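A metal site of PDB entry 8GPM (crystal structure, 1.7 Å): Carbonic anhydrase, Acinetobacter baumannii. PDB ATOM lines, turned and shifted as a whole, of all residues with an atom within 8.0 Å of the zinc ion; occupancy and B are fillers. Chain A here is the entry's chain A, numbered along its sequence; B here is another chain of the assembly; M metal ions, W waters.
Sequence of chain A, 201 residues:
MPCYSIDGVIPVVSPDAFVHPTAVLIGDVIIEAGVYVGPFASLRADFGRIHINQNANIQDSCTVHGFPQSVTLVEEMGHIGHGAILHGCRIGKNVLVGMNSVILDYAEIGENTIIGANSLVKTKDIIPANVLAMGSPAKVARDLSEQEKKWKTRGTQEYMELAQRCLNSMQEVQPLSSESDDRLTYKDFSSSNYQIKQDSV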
ATOM      1  N   ARG A  44      16.359  22.312  -5.533  1.00  0.00           N
ATOM      2  CA  ARG A  44      16.990  21.150  -6.177  1.00  0.00           C
ATOM      3  C   ARG A  44      16.234  19.904  -5.771  1.00  0.00           C
ATOM      4  O   ARG A  44      16.459  19.345  -4.689  1.00  0.00           O
ATOM      5  CB  ARG A  44      18.497  21.077  -5.844  1.00  0.00           C
ATOM      6  CG  ARG A  44      19.208  19.929  -6.623  1.00  0.00           C
ATOM      7  CD  ARG A  44      20.703  20.261  -6.825  1.00  0.00           C
ATOM      8  NE  ARG A  44      21.464  20.342  -5.571  1.00  0.00           N
ATOM      9  CZ  ARG A  44      22.144  19.338  -5.013  1.00  0.00           C
ATOM     10  NH1 ARG A  44      21.984  18.073  -5.440  1.00  0.00           N
ATOM     11  NH2 ARG A  44      22.959  19.595  -3.990  1.00  0.00           N
ATOM     12  N   ASP A  46      16.277  16.735  -6.979  1.00  0.00           N
ATOM     13  CA  ASP A  46      16.901  15.608  -7.661  1.00  0.00           C
ATOM     14  C   ASP A  46      17.011  14.362  -6.805  1.00  0.00           C
ATOM     15  O   ASP A  46      17.314  13.289  -7.332  1.00  0.00           O
ATOM     16  CB  ASP A  46      18.311  16.024  -8.170  1.00  0.00           C
ATOM     17  CG  ASP A  46      19.232  16.548  -7.065  1.00  0.00           C
ATOM     18  OD1 ASP A  46      18.866  16.504  -5.872  1.00  0.00           O
ATOM     19  OD2 ASP A  46      20.351  17.004  -7.411  1.00  0.00           O
ATOM     20  N   PHE A  47      16.744  14.488  -5.494  1.00  0.00           N
ATOM     21  CA  PHE A  47      16.602  13.323  -4.651  1.00  0.00           C
ATOM     22  C   PHE A  47      15.157  13.087  -4.225  1.00  0.00           C
ATOM     23  O   PHE A  47      14.716  11.934  -4.120  1.00  0.00           O
ATOM     24  CB  PHE A  47      17.473  13.463  -3.368  1.00  0.00           C
ATOM     25  CG  PHE A  47      18.982  13.387  -3.604  1.00  0.00           C
ATOM     26  CD1 PHE A  47      19.497  12.972  -4.817  1.00  0.00           C
ATOM     27  CD2 PHE A  47      19.859  13.717  -2.594  1.00  0.00           C
ATOM     28  CE1 PHE A  47      20.882  12.888  -5.013  1.00  0.00           C
ATOM     29  CE2 PHE A  47      21.229  13.648  -2.782  1.00  0.00           C
ATOM     30  CZ  PHE A  47      21.741  13.256  -3.993  1.00  0.00           C
ATOM     31  N   THR A  63      18.763  27.738  -0.458  1.00  0.00           N
ATOM     32  CA  THR A  63      18.827  26.393  -1.039  1.00  0.00           C
ATOM     33  C   THR A  63      17.739  25.552  -0.401  1.00  0.00           C
ATOM     34  O   THR A  63      17.538  25.597   0.817  1.00  0.00           O
ATOM     35  CB  THR A  63      20.197  25.741  -0.806  1.00  0.00           C
ATOM     36  OG1 THR A  63      21.198  26.520  -1.463  1.00  0.00           O
ATOM     37  CG2 THR A  63      20.239  24.297  -1.368  1.00  0.00           C
ATOM     38  N   VAL A  64      17.042  24.775  -1.224  1.00  0.00           N
ATOM     39  CA  VAL A  64      16.021  23.839  -0.761  1.00  0.00           C
ATOM     40  C   VAL A  64      16.436  22.501  -1.327  1.00  0.00           C
ATOM     41  O   VAL A  64      16.637  22.395  -2.549  1.00  0.00           O
ATOM     42  CB  VAL A  64      14.593  24.228  -1.180  1.00  0.00           C
ATOM     43  CG1 VAL A  64      13.567  23.228  -0.529  1.00  0.00           C
ATOM     44  CG2 VAL A  64      14.261  25.705  -0.816  1.00  0.00           C
ATOM     45  N   HIS A  65      16.647  21.512  -0.464  1.00  0.00           N
ATOM     46  CA  HIS A  65      17.093  20.187  -0.898  1.00  0.00           C
ATOM     47  C   HIS A  65      16.570  19.150   0.082  1.00  0.00           C
ATOM     48  O   HIS A  65      15.810  19.481   0.986  1.00  0.00           O
ATOM     49  CB  HIS A  65      18.633  20.126  -1.003  1.00  0.00           C
ATOM     50  CG  HIS A  65      19.153  18.955  -1.789  1.00  0.00           C
ATOM     51  ND1 HIS A  65      20.027  18.036  -1.278  1.00  0.00           N
ATOM     52  CD2 HIS A  65      18.879  18.534  -3.052  1.00  0.00           C
ATOM     53  CE1 HIS A  65      20.304  17.099  -2.177  1.00  0.00           C
ATOM     54  NE2 HIS A  65      19.623  17.389  -3.270  1.00  0.00           N
ATOM     55  N   GLY A  66      16.889  17.885  -0.163  1.00  0.00           N
ATOM     56  CA  GLY A  66      16.389  16.847   0.751  1.00  0.00           C
ATOM     57  C   GLY A  66      17.108  15.544   0.455  1.00  0.00           C
ATOM     58  O   GLY A  66      17.845  15.426  -0.521  1.00  0.00           O
ATOM     59  N   PHE A  67      16.870  14.554   1.319  1.00  0.00           N
ATOM     60  CA  PHE A  67      17.468  13.250   1.034  1.00  0.00           C
ATOM     61  C   PHE A  67      16.572  12.448   0.106  1.00  0.00           C
ATOM     62  O   PHE A  67      15.491  12.875  -0.302  1.00  0.00           O
ATOM     63  CB  PHE A  67      17.746  12.523   2.350  1.00  0.00           C
ATOM     64  CG  PHE A  67      18.976  13.036   3.044  1.00  0.00           C
ATOM     65  CD1 PHE A  67      20.190  13.102   2.379  1.00  0.00           C
ATOM     66  CD2 PHE A  67      18.912  13.505   4.341  1.00  0.00           C
ATOM     67  CE1 PHE A  67      21.315  13.601   2.999  1.00  0.00           C
ATOM     68  CE2 PHE A  67      20.045  13.993   4.960  1.00  0.00           C
ATOM     69  CZ  PHE A  67      21.233  14.047   4.302  1.00  0.00           C
ATOM     70  N   PRO A  68      17.049  11.280  -0.350  1.00  0.00           N
ATOM     71  CA  PRO A  68      16.281  10.500  -1.336  1.00  0.00           C
ATOM     72  C   PRO A  68      14.868  10.217  -0.858  1.00  0.00           C
ATOM     73  O   PRO A  68      14.635   9.767   0.272  1.00  0.00           O
ATOM     74  CB  PRO A  68      17.104   9.217  -1.471  1.00  0.00           C
ATOM     75  CG  PRO A  68      18.508   9.680  -1.239  1.00  0.00           C
ATOM     76  CD  PRO A  68      18.398  10.723  -0.150  1.00  0.00           C
ATOM     77  N   ILE A  85      18.707  27.747   4.382  1.00  0.00           N
ATOM     78  CA  ILE A  85      18.805  26.450   3.754  1.00  0.00           C
ATOM     79  C   ILE A  85      17.734  25.556   4.358  1.00  0.00           C
ATOM     80  O   ILE A  85      17.697  25.349   5.586  1.00  0.00           O
ATOM     81  CB  ILE A  85      20.198  25.842   3.977  1.00  0.00           C
ATOM     82  CG1 ILE A  85      21.262  26.740   3.304  1.00  0.00           C
ATOM     83  CG2 ILE A  85      20.227  24.410   3.457  1.00  0.00           C
ATOM     84  CD1 ILE A  85      22.716  26.456   3.751  1.00  0.00           C
ATOM     85  N   LEU A  86      16.876  24.989   3.517  1.00  0.00           N
ATOM     86  CA  LEU A  86      15.798  24.110   3.971  1.00  0.00           C
ATOM     87  C   LEU A  86      16.118  22.719   3.480  1.00  0.00           C
ATOM     88  O   LEU A  86      16.281  22.529   2.285  1.00  0.00           O
ATOM     89  CB  LEU A  86      14.446  24.538   3.403  1.00  0.00           C
ATOM     90  CG  LEU A  86      14.092  25.982   3.639  1.00  0.00           C
ATOM     91  CD1 LEU A  86      12.684  26.219   3.005  1.00  0.00           C
ATOM     92  CD2 LEU A  86      14.052  26.288   5.167  1.00  0.00           C
ATOM     93  N   HIS A  87      16.198  21.733   4.402  1.00  0.00           N
ATOM     94  CA  HIS A  87      16.629  20.390   4.020  1.00  0.00           C
ATOM     95  C   HIS A  87      15.622  19.377   4.546  1.00  0.00           C
ATOM     96  O   HIS A  87      15.661  19.022   5.722  1.00  0.00           O
ATOM     97  CB  HIS A  87      18.034  20.095   4.540  1.00  0.00           C
ATOM     98  CG  HIS A  87      18.759  19.145   3.674  1.00  0.00           C
ATOM     99  ND1 HIS A  87      18.615  17.774   3.808  1.00  0.00           N
ATOM    100  CD2 HIS A  87      19.552  19.337   2.592  1.00  0.00           C
ATOM    101  CE1 HIS A  87      19.364  17.162   2.909  1.00  0.00           C
ATOM    102  NE2 HIS A  87      19.911  18.090   2.153  1.00  0.00           N
ATOM    103  N   GLY A  88      14.729  18.913   3.669  1.00  0.00           N
ATOM    104  CA  GLY A  88      13.887  17.776   4.044  1.00  0.00           C
ATOM    105  C   GLY A  88      12.898  18.072   5.147  1.00  0.00           C
ATOM    106  O   GLY A  88      12.445  17.127   5.813  1.00  0.00           O
ATOM    107  N   ASP A 105      16.555  17.873   8.378  1.00  0.00           N
ATOM    108  CA  ASP A 105      15.588  16.929   7.859  1.00  0.00           C
ATOM    109  C   ASP A 105      14.579  16.517   8.889  1.00  0.00           C
ATOM    110  O   ASP A 105      14.917  16.284  10.052  1.00  0.00           O
ATOM    111  CB  ASP A 105      16.321  15.719   7.342  1.00  0.00           C
ATOM    112  CG  ASP A 105      17.393  16.134   6.376  1.00  0.00           C
ATOM    113  OD1 ASP A 105      18.497  16.554   6.813  1.00  0.00           O
ATOM    114  OD2 ASP A 105      17.080  16.108   5.171  1.00  0.00           O
ATOM    115  N   GLN B  59      28.420  21.428  -3.030  1.00  0.00           N
ATOM    116  CA  GLN B  59      26.976  21.607  -3.147  1.00  0.00           C
ATOM    117  C   GLN B  59      26.602  23.078  -3.366  1.00  0.00           C
ATOM    118  O   GLN B  59      27.450  23.940  -3.690  1.00  0.00           O
ATOM    119  CB  GLN B  59      26.281  21.026  -1.913  1.00  0.00           C
ATOM    120  CG  GLN B  59      26.533  19.505  -1.860  1.00  0.00           C
ATOM    121  CD  GLN B  59      25.987  18.881  -0.602  1.00  0.00           C
ATOM    122  OE1 GLN B  59      25.086  19.421   0.004  1.00  0.00           O
ATOM    123  NE2 GLN B  59      26.519  17.723  -0.220  1.00  0.00           N
ATOM    124  N   ASP B  60      25.311  23.354  -3.248  1.00  0.00           N
ATOM    125  CA  ASP B  60      24.754  24.567  -3.844  1.00  0.00           C
ATOM    126  C   ASP B  60      25.241  25.819  -3.116  1.00  0.00           C
ATOM    127  O   ASP B  60      25.269  25.869  -1.872  1.00  0.00           O
ATOM    128  CB  ASP B  60      23.233  24.613  -3.789  1.00  0.00           C
ATOM    129  CG  ASP B  60      22.574  23.264  -4.066  1.00  0.00           C
ATOM    130  OD1 ASP B  60      22.920  22.326  -3.310  1.00  0.00           O
ATOM    131  OD2 ASP B  60      21.845  23.141  -5.087  1.00  0.00           O
ATOM    132  N   HIS B  79      32.883  15.886   0.948  1.00  0.00           N
ATOM    133  CA  HIS B  79      31.439  16.035   0.782  1.00  0.00           C
ATOM    134  C   HIS B  79      31.125  17.390   1.387  1.00  0.00           C
ATOM    135  O   HIS B  79      31.063  17.527   2.604  1.00  0.00           O
ATOM    136  CB  HIS B  79      30.737  14.851   1.490  1.00  0.00           C
ATOM    137  CG  HIS B  79      29.250  14.742   1.318  1.00  0.00           C
ATOM    138  ND1 HIS B  79      28.652  13.612   0.782  1.00  0.00           N
ATOM    139  CD2 HIS B  79      28.234  15.562   1.696  1.00  0.00           C
ATOM    140  CE1 HIS B  79      27.337  13.761   0.796  1.00  0.00           C
ATOM    141  NE2 HIS B  79      27.053  14.934   1.345  1.00  0.00           N
ATOM    142  N   GLY B  81      28.839  20.382   2.162  1.00  0.00           N
ATOM    143  CA  GLY B  81      27.407  20.620   2.257  1.00  0.00           C
ATOM    144  C   GLY B  81      26.987  22.008   1.816  1.00  0.00           C
ATOM    145  O   GLY B  81      27.759  22.936   1.776  1.00  0.00           O
ATOM    146  N   HIS B  82      25.689  22.120   1.472  1.00  0.00           N
ATOM    147  CA  HIS B  82      25.118  23.377   0.931  1.00  0.00           C
ATOM    148  C   HIS B  82      25.637  24.599   1.660  1.00  0.00           C
ATOM    149  O   HIS B  82      25.509  24.696   2.887  1.00  0.00           O
ATOM    150  CB  HIS B  82      23.599  23.343   1.069  1.00  0.00           C
ATOM    151  CG  HIS B  82      22.976  22.052   0.624  1.00  0.00           C
ATOM    152  ND1 HIS B  82      22.714  21.790  -0.711  1.00  0.00           N
ATOM    153  CD2 HIS B  82      22.488  21.006   1.327  1.00  0.00           C
ATOM    154  CE1 HIS B  82      22.138  20.594  -0.817  1.00  0.00           C
ATOM    155  NE2 HIS B  82      22.018  20.099   0.405  1.00  0.00           N
ATOM    156  N   MET B  99      26.437  21.712   6.245  1.00  0.00           N
ATOM    157  CA  MET B  99      25.854  22.898   5.632  1.00  0.00           C
ATOM    158  C   MET B  99      26.163  24.198   6.350  1.00  0.00           C
ATOM    159  O   MET B  99      26.108  24.286   7.581  1.00  0.00           O
ATOM    160  CB  MET B  99      24.340  22.730   5.487  1.00  0.00           C
ATOM    161  CG  MET B  99      23.891  21.403   4.936  1.00  0.00           C
ATOM    162  SD  MET B  99      22.066  21.373   5.102  1.00  0.00           S
ATOM    163  CE  MET B  99      21.950  19.596   5.200  1.00  0.00           C
ATOM    164  N   TYR B 159      25.847  11.020  -4.125  1.00  0.00           N
ATOM    165  CA  TYR B 159      26.340  12.114  -4.965  1.00  0.00           C
ATOM    166  C   TYR B 159      27.199  11.606  -6.111  1.00  0.00           C
ATOM    167  O   TYR B 159      27.253  12.242  -7.178  1.00  0.00           O
ATOM    168  CB  TYR B 159      27.135  13.158  -4.157  1.00  0.00           C
ATOM    169  CG  TYR B 159      26.236  14.249  -3.655  1.00  0.00           C
ATOM    170  CD1 TYR B 159      25.552  14.121  -2.456  1.00  0.00           C
ATOM    171  CD2 TYR B 159      26.029  15.418  -4.397  1.00  0.00           C
ATOM    172  CE1 TYR B 159      24.688  15.112  -1.993  1.00  0.00           C
ATOM    173  CE2 TYR B 159      25.164  16.448  -3.908  1.00  0.00           C
ATOM    174  CZ  TYR B 159      24.504  16.271  -2.738  1.00  0.00           C
ATOM    175  OH  TYR B 159      23.631  17.243  -2.246  1.00  0.00           O
HETATM  176 ZN    ZN M   1      21.200  18.146   0.498  1.00  0.00          ZN
HETATM  177  O   HOH W   1      22.663  16.807   0.254  1.00  0.00           O
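Residues that only touch the zinc ion: Tyr 159 of chain B.
Four residues have an atom within 4 Å of the zinc ion: His 65, His 87, His 82 of chain B and Tyr 159 of chain B.
The nearest printed residue that does not touch the zinc ion is Gln 59 of chain B (4.1 Å).
OD2 of Asp 105 is in hydrogen-bond range of ND1 of His 87 (2.6 Å).
The side-chain amide oxygen of Gln 59 of chain B lies within hydrogen-bond range of the backbone NH of His 82 of chain B.
A ring nitrogen (NE2) of His 65 is in hydrogen-bond range of the guanidinium group of Arg 44.
O of Leu 86 is in hydrogen-bond range of N of His 65, at 3.0 Å.
The side-chain carboxylate of Asp 46 is in hydrogen-bond range of a ring nitrogen (NE2) of His 65, 2.9 Å away.
O of His 65 lies within hydrogen-bond range of N of Gly 88, 2.9 Å away.
OE1 of Gln 59 of chain B sits close to OH of Tyr 159 of chain B, at 3.5 Å.
The side-chain hydroxyl of Tyr 159 of chain B sits at hydrogen-bond distance from the guanidinium group of Arg 44, 3.0 Å away.
The zinc ion is bound by water W1 (2.0 Å).
The zinc ion is bound by a ring nitrogen (NE2) of His 87, at 2.1 Å.
The zinc ion is bound by a ring nitrogen (NE2) of His 82 of chain B, at 2.1 Å.
A ring nitrogen (ND1) of His 65 binds the zinc ion.
The zinc ion has four donor atoms within binding distance.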
